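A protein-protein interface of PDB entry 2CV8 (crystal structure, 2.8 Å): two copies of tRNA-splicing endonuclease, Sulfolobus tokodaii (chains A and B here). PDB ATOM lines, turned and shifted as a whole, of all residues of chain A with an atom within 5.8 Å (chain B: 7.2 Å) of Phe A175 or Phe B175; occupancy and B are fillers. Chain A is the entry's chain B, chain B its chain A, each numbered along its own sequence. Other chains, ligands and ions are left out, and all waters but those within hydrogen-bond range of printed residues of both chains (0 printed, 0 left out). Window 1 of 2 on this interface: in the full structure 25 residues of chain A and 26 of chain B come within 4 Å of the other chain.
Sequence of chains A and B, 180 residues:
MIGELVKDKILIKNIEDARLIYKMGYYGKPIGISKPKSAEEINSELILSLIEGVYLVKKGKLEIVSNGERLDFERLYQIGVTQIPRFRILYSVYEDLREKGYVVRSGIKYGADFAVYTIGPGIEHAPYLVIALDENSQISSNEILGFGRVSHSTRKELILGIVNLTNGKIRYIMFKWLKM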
ATOM      1  N   ILE A 144      -5.106 -33.489  19.892  1.00  0.00           N
ATOM      2  CA  ILE A 144      -6.070 -32.473  20.293  1.00  0.00           C
ATOM      3  C   ILE A 144      -6.546 -32.798  21.706  1.00  0.00           C
ATOM      4  O   ILE A 144      -6.735 -31.898  22.523  1.00  0.00           O
ATOM      5  CB  ILE A 144      -7.279 -32.400  19.306  1.00  0.00           C
ATOM      6  CG1 ILE A 144      -6.837 -31.735  18.006  1.00  0.00           C
ATOM      7  CG2 ILE A 144      -8.437 -31.586  19.909  1.00  0.00           C
ATOM      8  CD1 ILE A 144      -7.996 -31.467  17.042  1.00  0.00           C
ATOM      9  N   PHE A 147      -4.006 -31.799  24.044  1.00  0.00           N
ATOM     10  CA  PHE A 147      -4.023 -30.348  24.194  1.00  0.00           C
ATOM     11  C   PHE A 147      -4.899 -30.023  25.397  1.00  0.00           C
ATOM     12  O   PHE A 147      -4.405 -29.560  26.424  1.00  0.00           O
ATOM     13  CB  PHE A 147      -4.631 -29.683  22.949  1.00  0.00           C
ATOM     14  CG  PHE A 147      -3.671 -29.516  21.786  1.00  0.00           C
ATOM     15  CD1 PHE A 147      -4.161 -29.194  20.519  1.00  0.00           C
ATOM     16  CD2 PHE A 147      -2.288 -29.636  21.960  1.00  0.00           C
ATOM     17  CE1 PHE A 147      -3.295 -28.990  19.445  1.00  0.00           C
ATOM     18  CE2 PHE A 147      -1.405 -29.431  20.883  1.00  0.00           C
ATOM     19  CZ  PHE A 147      -1.915 -29.107  19.625  1.00  0.00           C
ATOM     20  N   GLY A 148      -6.200 -30.285  25.259  1.00  0.00           N
ATOM     21  CA  GLY A 148      -7.160 -30.022  26.322  1.00  0.00           C
ATOM     22  C   GLY A 148      -6.878 -30.706  27.650  1.00  0.00           C
ATOM     23  O   GLY A 148      -7.672 -30.619  28.587  1.00  0.00           O
ATOM     24  N   SER A 151      -4.293 -28.131  29.256  1.00  0.00           N
ATOM     25  CA  SER A 151      -5.106 -26.961  29.563  1.00  0.00           C
ATOM     26  C   SER A 151      -5.658 -26.999  30.991  1.00  0.00           C
ATOM     27  O   SER A 151      -5.181 -26.274  31.865  1.00  0.00           O
ATOM     28  CB  SER A 151      -6.251 -26.843  28.552  1.00  0.00           C
ATOM     29  OG  SER A 151      -6.743 -25.514  28.488  1.00  0.00           O
ATOM     30  N   LEU A 158      -4.987 -21.989  27.591  1.00  0.00           N
ATOM     31  CA  LEU A 158      -4.277 -22.660  26.503  1.00  0.00           C
ATOM     32  C   LEU A 158      -4.620 -21.963  25.189  1.00  0.00           C
ATOM     33  O   LEU A 158      -5.785 -21.663  24.913  1.00  0.00           O
ATOM     34  CB  LEU A 158      -4.676 -24.135  26.437  1.00  0.00           C
ATOM     35  CG  LEU A 158      -3.811 -25.047  25.563  1.00  0.00           C
ATOM     36  CD1 LEU A 158      -3.974 -24.661  24.110  1.00  0.00           C
ATOM     37  CD2 LEU A 158      -2.348 -24.951  25.986  1.00  0.00           C
ATOM     38  N   ILE A 159      -3.602 -21.730  24.366  1.00  0.00           N
ATOM     39  CA  ILE A 159      -3.786 -21.028  23.098  1.00  0.00           C
ATOM     40  C   ILE A 159      -2.899 -21.560  21.979  1.00  0.00           C
ATOM     41  O   ILE A 159      -1.709 -21.786  22.173  1.00  0.00           O
ATOM     42  CB  ILE A 159      -3.504 -19.516  23.287  1.00  0.00           C
ATOM     43  CG1 ILE A 159      -4.529 -18.922  24.247  1.00  0.00           C
ATOM     44  CG2 ILE A 159      -3.574 -18.782  21.962  1.00  0.00           C
ATOM     45  CD1 ILE A 159      -4.394 -17.439  24.431  1.00  0.00           C
ATOM     46  N   LEU A 160      -3.503 -21.749  20.809  1.00  0.00           N
ATOM     47  CA  LEU A 160      -2.822 -22.250  19.620  1.00  0.00           C
ATOM     48  C   LEU A 160      -2.313 -21.097  18.774  1.00  0.00           C
ATOM     49  O   LEU A 160      -3.076 -20.212  18.401  1.00  0.00           O
ATOM     50  CB  LEU A 160      -3.792 -23.097  18.789  1.00  0.00           C
ATOM     51  CG  LEU A 160      -3.640 -24.615  18.850  1.00  0.00           C
ATOM     52  CD1 LEU A 160      -2.403 -24.997  18.062  1.00  0.00           C
ATOM     53  CD2 LEU A 160      -3.525 -25.093  20.288  1.00  0.00           C
ATOM     54  N   ILE A 173      -5.926 -19.118  18.291  1.00  0.00           N
ATOM     55  CA  ILE A 173      -7.192 -19.740  18.614  1.00  0.00           C
ATOM     56  C   ILE A 173      -7.024 -20.442  19.945  1.00  0.00           C
ATOM     57  O   ILE A 173      -6.138 -21.278  20.123  1.00  0.00           O
ATOM     58  CB  ILE A 173      -7.664 -20.738  17.499  1.00  0.00           C
ATOM     59  CG1 ILE A 173      -7.106 -22.140  17.737  1.00  0.00           C
ATOM     60  CG2 ILE A 173      -7.192 -20.251  16.125  1.00  0.00           C
ATOM     61  CD1 ILE A 173      -7.787 -23.215  16.895  1.00  0.00           C
ATOM     62  N   MET A 174      -7.865 -20.067  20.893  1.00  0.00           N
ATOM     63  CA  MET A 174      -7.819 -20.638  22.225  1.00  0.00           C
ATOM     64  C   MET A 174      -8.925 -21.650  22.406  1.00  0.00           C
ATOM     65  O   MET A 174      -9.991 -21.493  21.823  1.00  0.00           O
ATOM     66  CB  MET A 174      -8.007 -19.534  23.255  1.00  0.00           C
ATOM     67  CG  MET A 174      -8.389 -20.024  24.639  1.00  0.00           C
ATOM     68  SD  MET A 174      -9.726 -18.865  25.409  1.00  0.00           S
ATOM     69  CE  MET A 174     -11.295 -19.778  24.783  1.00  0.00           C
ATOM     70  N   PHE A 175      -8.675 -22.689  23.202  1.00  0.00           N
ATOM     71  CA  PHE A 175      -9.718 -23.669  23.467  1.00  0.00           C
ATOM     72  C   PHE A 175      -9.686 -24.197  24.882  1.00  0.00           C
ATOM     73  O   PHE A 175      -8.623 -24.322  25.483  1.00  0.00           O
ATOM     74  CB  PHE A 175      -9.692 -24.836  22.468  1.00  0.00           C
ATOM     75  CG  PHE A 175      -8.347 -25.449  22.261  1.00  0.00           C
ATOM     76  CD1 PHE A 175      -7.538 -25.777  23.337  1.00  0.00           C
ATOM     77  CD2 PHE A 175      -7.912 -25.744  20.975  1.00  0.00           C
ATOM     78  CE1 PHE A 175      -6.321 -26.390  23.139  1.00  0.00           C
ATOM     79  CE2 PHE A 175      -6.693 -26.358  20.767  1.00  0.00           C
ATOM     80  CZ  PHE A 175      -5.894 -26.683  21.852  1.00  0.00           C
ATOM     81  N   LYS A 176     -10.872 -24.491  25.405  1.00  0.00           N
ATOM     82  CA  LYS A 176     -11.024 -24.993  26.752  1.00  0.00           C
ATOM     83  C   LYS A 176     -11.654 -26.369  26.740  1.00  0.00           C
ATOM     84  O   LYS A 176     -12.379 -26.712  25.818  1.00  0.00           O
ATOM     85  CB  LYS A 176     -11.914 -24.053  27.563  1.00  0.00           C
ATOM     86  CG  LYS A 176     -11.440 -22.617  27.580  1.00  0.00           C
ATOM     87  CD  LYS A 176     -12.276 -21.785  28.523  1.00  0.00           C
ATOM     88  CE  LYS A 176     -11.732 -20.378  28.647  1.00  0.00           C
ATOM     89  NZ  LYS A 176     -12.481 -19.598  29.671  1.00  0.00           N
ATOM     90  N   TRP A 177     -11.358 -27.155  27.768  1.00  0.00           N
ATOM     91  CA  TRP A 177     -11.928 -28.480  27.921  1.00  0.00           C
ATOM     92  C   TRP A 177     -13.306 -28.201  28.536  1.00  0.00           C
ATOM     93  O   TRP A 177     -13.405 -27.715  29.664  1.00  0.00           O
ATOM     94  CB  TRP A 177     -11.060 -29.304  28.878  1.00  0.00           C
ATOM     95  CG  TRP A 177     -11.491 -30.733  29.052  1.00  0.00           C
ATOM     96  CD1 TRP A 177     -11.400 -31.736  28.131  1.00  0.00           C
ATOM     97  CD2 TRP A 177     -12.073 -31.319  30.228  1.00  0.00           C
ATOM     98  NE1 TRP A 177     -11.886 -32.911  28.657  1.00  0.00           N
ATOM     99  CE2 TRP A 177     -12.307 -32.683  29.942  1.00  0.00           C
ATOM    100  CE3 TRP A 177     -12.423 -30.822  31.494  1.00  0.00           C
ATOM    101  CZ2 TRP A 177     -12.874 -33.561  30.877  1.00  0.00           C
ATOM    102  CZ3 TRP A 177     -12.986 -31.694  32.422  1.00  0.00           C
ATOM    103  CH2 TRP A 177     -13.205 -33.049  32.107  1.00  0.00           C
ATOM    104  N   ILE B 131     -19.078 -30.073  15.777  1.00  0.00           N
ATOM    105  CA  ILE B 131     -18.618 -30.959  14.732  1.00  0.00           C
ATOM    106  C   ILE B 131     -18.135 -32.217  15.440  1.00  0.00           C
ATOM    107  O   ILE B 131     -17.191 -32.174  16.224  1.00  0.00           O
ATOM    108  CB  ILE B 131     -17.472 -30.328  13.925  1.00  0.00           C
ATOM    109  CG1 ILE B 131     -18.049 -29.343  12.907  1.00  0.00           C
ATOM    110  CG2 ILE B 131     -16.656 -31.414  13.241  1.00  0.00           C
ATOM    111  CD1 ILE B 131     -17.008 -28.525  12.169  1.00  0.00           C
ATOM    112  N   ILE B 139      -7.654 -33.534  11.701  1.00  0.00           N
ATOM    113  CA  ILE B 139      -8.082 -32.250  11.165  1.00  0.00           C
ATOM    114  C   ILE B 139      -6.904 -31.277  11.129  1.00  0.00           C
ATOM    115  O   ILE B 139      -6.084 -31.225  12.051  1.00  0.00           O
ATOM    116  CB  ILE B 139      -9.221 -31.649  12.009  1.00  0.00           C
ATOM    117  CG1 ILE B 139      -9.797 -30.433  11.296  1.00  0.00           C
ATOM    118  CG2 ILE B 139      -8.714 -31.240  13.386  1.00  0.00           C
ATOM    119  CD1 ILE B 139     -10.990 -29.827  12.010  1.00  0.00           C
ATOM    120  N   GLU B 143      -8.219 -26.231   8.861  1.00  0.00           N
ATOM    121  CA  GLU B 143      -9.506 -26.840   8.529  1.00  0.00           C
ATOM    122  C   GLU B 143     -10.402 -26.362   9.666  1.00  0.00           C
ATOM    123  O   GLU B 143     -11.572 -26.035   9.477  1.00  0.00           O
ATOM    124  CB  GLU B 143      -9.410 -28.372   8.522  1.00  0.00           C
ATOM    125  CG  GLU B 143      -8.502 -28.918   7.430  1.00  0.00           C
ATOM    126  CD  GLU B 143      -8.638 -30.415   7.225  1.00  0.00           C
ATOM    127  OE1 GLU B 143      -8.481 -31.179   8.197  1.00  0.00           O
ATOM    128  OE2 GLU B 143      -8.900 -30.828   6.078  1.00  0.00           O
ATOM    129  N   ILE B 144      -9.800 -26.305  10.848  1.00  0.00           N
ATOM    130  CA  ILE B 144     -10.445 -25.843  12.064  1.00  0.00           C
ATOM    131  C   ILE B 144     -10.881 -24.387  11.883  1.00  0.00           C
ATOM    132  O   ILE B 144     -11.991 -24.120  11.421  1.00  0.00           O
ATOM    133  CB  ILE B 144      -9.460 -25.926  13.239  1.00  0.00           C
ATOM    134  CG1 ILE B 144      -9.147 -27.390  13.544  1.00  0.00           C
ATOM    135  CG2 ILE B 144     -10.012 -25.198  14.438  1.00  0.00           C
ATOM    136  CD1 ILE B 144      -8.084 -27.584  14.601  1.00  0.00           C
ATOM    137  N   LEU B 145     -10.003 -23.448  12.240  1.00  0.00           N
ATOM    138  CA  LEU B 145     -10.319 -22.033  12.105  1.00  0.00           C
ATOM    139  C   LEU B 145     -10.825 -21.821  10.686  1.00  0.00           C
ATOM    140  O   LEU B 145     -11.538 -20.857  10.402  1.00  0.00           O
ATOM    141  CB  LEU B 145      -9.080 -21.166  12.385  1.00  0.00           C
ATOM    142  CG  LEU B 145      -7.863 -21.192  11.453  1.00  0.00           C
ATOM    143  CD1 LEU B 145      -8.149 -20.403  10.185  1.00  0.00           C
ATOM    144  CD2 LEU B 145      -6.670 -20.582  12.166  1.00  0.00           C
ATOM    145  N   VAL B 150     -15.911 -19.811  12.369  1.00  0.00           N
ATOM    146  CA  VAL B 150     -14.658 -19.249  12.847  1.00  0.00           C
ATOM    147  C   VAL B 150     -14.138 -18.443  11.665  1.00  0.00           C
ATOM    148  O   VAL B 150     -14.232 -18.896  10.521  1.00  0.00           O
ATOM    149  CB  VAL B 150     -13.643 -20.367  13.175  1.00  0.00           C
ATOM    150  CG1 VAL B 150     -12.317 -19.767  13.610  1.00  0.00           C
ATOM    151  CG2 VAL B 150     -14.209 -21.281  14.253  1.00  0.00           C
ATOM    152  N   LYS B 156     -16.585 -16.322  15.548  1.00  0.00           N
ATOM    153  CA  LYS B 156     -17.271 -16.916  16.686  1.00  0.00           C
ATOM    154  C   LYS B 156     -16.683 -18.277  17.061  1.00  0.00           C
ATOM    155  O   LYS B 156     -15.550 -18.593  16.690  1.00  0.00           O
ATOM    156  CB  LYS B 156     -18.775 -17.038  16.401  1.00  0.00           C
ATOM    157  CG  LYS B 156     -19.146 -18.011  15.299  1.00  0.00           C
ATOM    158  CD  LYS B 156     -20.613 -17.865  14.876  1.00  0.00           C
ATOM    159  CE  LYS B 156     -20.848 -16.597  14.048  1.00  0.00           C
ATOM    160  NZ  LYS B 156     -22.226 -16.526  13.460  1.00  0.00           N
ATOM    161  N   GLU B 157     -17.459 -19.084  17.782  1.00  0.00           N
ATOM    162  CA  GLU B 157     -16.998 -20.389  18.254  1.00  0.00           C
ATOM    163  C   GLU B 157     -17.431 -21.615  17.455  1.00  0.00           C
ATOM    164  O   GLU B 157     -18.402 -21.582  16.695  1.00  0.00           O
ATOM    165  CB  GLU B 157     -17.453 -20.606  19.697  1.00  0.00           C
ATOM    166  CG  GLU B 157     -17.151 -19.475  20.646  1.00  0.00           C
ATOM    167  CD  GLU B 157     -18.399 -18.913  21.289  1.00  0.00           C
ATOM    168  OE1 GLU B 157     -19.339 -19.696  21.540  1.00  0.00           O
ATOM    169  OE2 GLU B 157     -18.434 -17.691  21.556  1.00  0.00           O
ATOM    170  N   LEU B 158     -16.711 -22.709  17.684  1.00  0.00           N
ATOM    171  CA  LEU B 158     -16.982 -23.994  17.048  1.00  0.00           C
ATOM    172  C   LEU B 158     -16.613 -25.063  18.087  1.00  0.00           C
ATOM    173  O   LEU B 158     -15.464 -25.098  18.522  1.00  0.00           O
ATOM    174  CB  LEU B 158     -16.117 -24.132  15.787  1.00  0.00           C
ATOM    175  CG  LEU B 158     -16.308 -25.280  14.782  1.00  0.00           C
ATOM    176  CD1 LEU B 158     -15.809 -26.571  15.376  1.00  0.00           C
ATOM    177  CD2 LEU B 158     -17.773 -25.392  14.376  1.00  0.00           C
ATOM    178  N   ILE B 159     -17.573 -25.893  18.521  1.00  0.00           N
ATOM    179  CA  ILE B 159     -17.273 -26.941  19.506  1.00  0.00           C
ATOM    180  C   ILE B 159     -16.966 -28.288  18.843  1.00  0.00           C
ATOM    181  O   ILE B 159     -17.714 -28.769  17.984  1.00  0.00           O
ATOM    182  CB  ILE B 159     -18.432 -27.150  20.531  1.00  0.00           C
ATOM    183  CG1 ILE B 159     -18.613 -25.897  21.385  1.00  0.00           C
ATOM    184  CG2 ILE B 159     -18.122 -28.338  21.446  1.00  0.00           C
ATOM    185  CD1 ILE B 159     -19.657 -26.045  22.476  1.00  0.00           C
ATOM    186  N   LEU B 160     -15.851 -28.883  19.263  1.00  0.00           N
ATOM    187  CA  LEU B 160     -15.388 -30.178  18.759  1.00  0.00           C
ATOM    188  C   LEU B 160     -15.915 -31.323  19.597  1.00  0.00           C
ATOM    189  O   LEU B 160     -15.708 -31.349  20.809  1.00  0.00           O
ATOM    190  CB  LEU B 160     -13.865 -30.229  18.779  1.00  0.00           C
ATOM    191  CG  LEU B 160     -13.141 -30.048  17.449  1.00  0.00           C
ATOM    192  CD1 LEU B 160     -13.281 -31.311  16.634  1.00  0.00           C
ATOM    193  CD2 LEU B 160     -13.717 -28.864  16.697  1.00  0.00           C
ATOM    194  N   ILE B 173     -14.481 -30.041  23.293  1.00  0.00           N
ATOM    195  CA  ILE B 173     -13.499 -28.974  23.398  1.00  0.00           C
ATOM    196  C   ILE B 173     -13.900 -27.860  22.436  1.00  0.00           C
ATOM    197  O   ILE B 173     -14.074 -28.075  21.235  1.00  0.00           O
ATOM    198  CB  ILE B 173     -12.055 -29.473  23.097  1.00  0.00           C
ATOM    199  CG1 ILE B 173     -11.750 -29.384  21.609  1.00  0.00           C
ATOM    200  CG2 ILE B 173     -11.896 -30.920  23.555  1.00  0.00           C
ATOM    201  CD1 ILE B 173     -10.282 -29.522  21.303  1.00  0.00           C
ATOM    202  N   MET B 174     -14.085 -26.670  22.992  1.00  0.00           N
ATOM    203  CA  MET B 174     -14.497 -25.510  22.217  1.00  0.00           C
ATOM    204  C   MET B 174     -13.318 -24.604  21.971  1.00  0.00           C
ATOM    205  O   MET B 174     -12.428 -24.511  22.810  1.00  0.00           O
ATOM    206  CB  MET B 174     -15.560 -24.729  22.986  1.00  0.00           C
ATOM    207  CG  MET B 174     -15.774 -23.319  22.484  1.00  0.00           C
ATOM    208  SD  MET B 174     -16.031 -22.105  23.938  1.00  0.00           S
ATOM    209  CE  MET B 174     -14.168 -21.640  24.234  1.00  0.00           C
ATOM    210  N   PHE B 175     -13.298 -23.948  20.817  1.00  0.00           N
ATOM    211  CA  PHE B 175     -12.226 -23.009  20.534  1.00  0.00           C
ATOM    212  C   PHE B 175     -12.692 -21.783  19.769  1.00  0.00           C
ATOM    213  O   PHE B 175     -13.595 -21.854  18.936  1.00  0.00           O
ATOM    214  CB  PHE B 175     -11.053 -23.674  19.806  1.00  0.00           C
ATOM    215  CG  PHE B 175     -11.442 -24.492  18.629  1.00  0.00           C
ATOM    216  CD1 PHE B 175     -12.350 -24.008  17.695  1.00  0.00           C
ATOM    217  CD2 PHE B 175     -10.874 -25.743  18.435  1.00  0.00           C
ATOM    218  CE1 PHE B 175     -12.688 -24.758  16.581  1.00  0.00           C
ATOM    219  CE2 PHE B 175     -11.201 -26.504  17.329  1.00  0.00           C
ATOM    220  CZ  PHE B 175     -12.113 -26.012  16.396  1.00  0.00           C
ATOM    221  N   LYS B 176     -12.066 -20.653  20.085  1.00  0.00           N
ATOM    222  CA  LYS B 176     -12.381 -19.378  19.465  1.00  0.00           C
ATOM    223  C   LYS B 176     -11.193 -18.821  18.707  1.00  0.00           C
ATOM    224  O   LYS B 176     -10.042 -19.088  19.054  1.00  0.00           O
ATOM    225  CB  LYS B 176     -12.782 -18.366  20.530  1.00  0.00           C
ATOM    226  CG  LYS B 176     -13.889 -18.828  21.441  1.00  0.00           C
ATOM    227  CD  LYS B 176     -14.321 -17.705  22.359  1.00  0.00           C
ATOM    228  CE  LYS B 176     -15.530 -18.104  23.182  1.00  0.00           C
ATOM    229  NZ  LYS B 176     -16.033 -16.970  24.002  1.00  0.00           N
ATOM    230  N   TRP B 177     -11.483 -18.050  17.666  1.00  0.00           N
ATOM    231  CA  TRP B 177     -10.448 -17.405  16.879  1.00  0.00           C
ATOM    232  C   TRP B 177     -10.062 -16.176  17.722  1.00  0.00           C
ATOM    233  O   TRP B 177     -10.865 -15.262  17.917  1.00  0.00           O
ATOM    234  CB  TRP B 177     -11.021 -16.983  15.525  1.00  0.00           C
ATOM    235  CG  TRP B 177     -10.021 -16.395  14.567  1.00  0.00           C
ATOM    236  CD1 TRP B 177      -9.025 -17.057  13.910  1.00  0.00           C
ATOM    237  CD2 TRP B 177      -9.930 -15.025  14.155  1.00  0.00           C
ATOM    238  NE1 TRP B 177      -8.319 -16.186  13.113  1.00  0.00           N
ATOM    239  CE2 TRP B 177      -8.852 -14.933  13.245  1.00  0.00           C
ATOM    240  CE3 TRP B 177     -10.655 -13.864  14.468  1.00  0.00           C
ATOM    241  CZ2 TRP B 177      -8.481 -13.729  12.644  1.00  0.00           C
ATOM    242  CZ3 TRP B 177     -10.287 -12.667  13.871  1.00  0.00           C
ATOM    243  CH2 TRP B 177      -9.207 -12.610  12.968  1.00  0.00           C
ATOM    244  N   LEU B 178      -8.843 -16.172  18.248  1.00  0.00           N
ATOM    245  CA  LEU B 178      -8.366 -15.070  19.082  1.00  0.00           C
ATOM    246  C   LEU B 178      -7.701 -13.948  18.306  1.00  0.00           C
ATOM    247  O   LEU B 178      -7.230 -14.132  17.181  1.00  0.00           O
ATOM    248  CB  LEU B 178      -7.368 -15.576  20.131  1.00  0.00           C
ATOM    249  CG  LEU B 178      -7.884 -16.294  21.376  1.00  0.00           C
ATOM    250  CD1 LEU B 178      -6.708 -16.806  22.186  1.00  0.00           C
ATOM    251  CD2 LEU B 178      -8.725 -15.340  22.200  1.00  0.00           C
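N of Lys A176 sits at hydrogen-bond distance from O of Met B174, 3.0 Å away. The backbone NH of Lys B176 is in hydrogen-bond range of the backbone carbonyl oxygen of Met A174.
Ile A144 touches Ile B173, and with the chains exchanged Ile A173 touches Ile B144. Met B174 touches its own counterpart, Met A174. Met A174 touches Phe B175, and with the chains exchanged Phe A175 touches Met B174. Met A174 touches Lys B176, and with the chains exchanged Lys A176 touches Met B174. Positions printed for both chains: 144, 158, 159, 160, 173, 174, 175, 176 and 177.
OE2 of Glu B157 is in salt-bridge range of NZ of Lys B176. The backbone carbonyl oxygen (O) of Leu B158 sits at hydrogen-bond distance from the backbone NH (N) of Phe B175. The backbone NH (N) of Leu B160 is in hydrogen-bond range of the backbone carbonyl oxygen (O) of Ile B173, at 2.8 Å. The backbone NH of Leu A160 sits at hydrogen-bond distance from the backbone carbonyl oxygen of Ile A173, 2.8 Å away.
Phe A175 touches two residues of chain B. Phe B175 touches two residues of chain A. Of the printed residues of chain A, Ile B139 touches Ile A144. Printed residues of chain A within 4 Å of Met B174: Met A174 (3.5 Å), Phe A175 (2.8 Å) and Lys A176 (3.0 Å). Of the printed residues of chain B, Met A174 touches Met B174 (3.5 Å), Phe B175 (3.0 Å), Lys B176 (2.8 Å) and Leu B178 (3.2 Å). Of the printed residues of chain A, Lys B176 touches Ile A173 and Met A174. Trp A177 touches none of the printed residues of chain B. The nearest residue of chain B that does not touch Phe A175 is Ile B173 (4.5 Å). The nearest residue of chain A that does not touch Phe B175 is Ile A173 (4.2 Å).
Of the 12 printed residues of chain A, 6 touch a printed residue of chain B. Printed residues of chain A that touch a printed residue of chain B: Ile A144, Ile A159, Ile A173, Met A174, Phe A175 and Lys A176. Among the printed residues, no Asp or Glu carboxylate lies within 4 Å of a Lys or Arg side-chain nitrogen of the other chain.
Ile A144 touches Ile B139 (CD1 to CG2, 3.7 Å). Ile B173 touches Ile A144 (CD1 to CG2, 3.1 Å). Ile A159 touches Leu B178 (CD1 to CD1, 3.3 Å). Ile A173 touches Ile B144. Lys B176 touches Ile A173. Met A174 touches Met B174 (CE to CE, 3.5 Å). CB of Met A174 touches CD1 of Leu B178 (3.2 Å). Phe A175 touches Met B174. Phe A175 touches Phe B175 (CB to CB, 3.2 Å). Lys A176 touches Ile B173.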
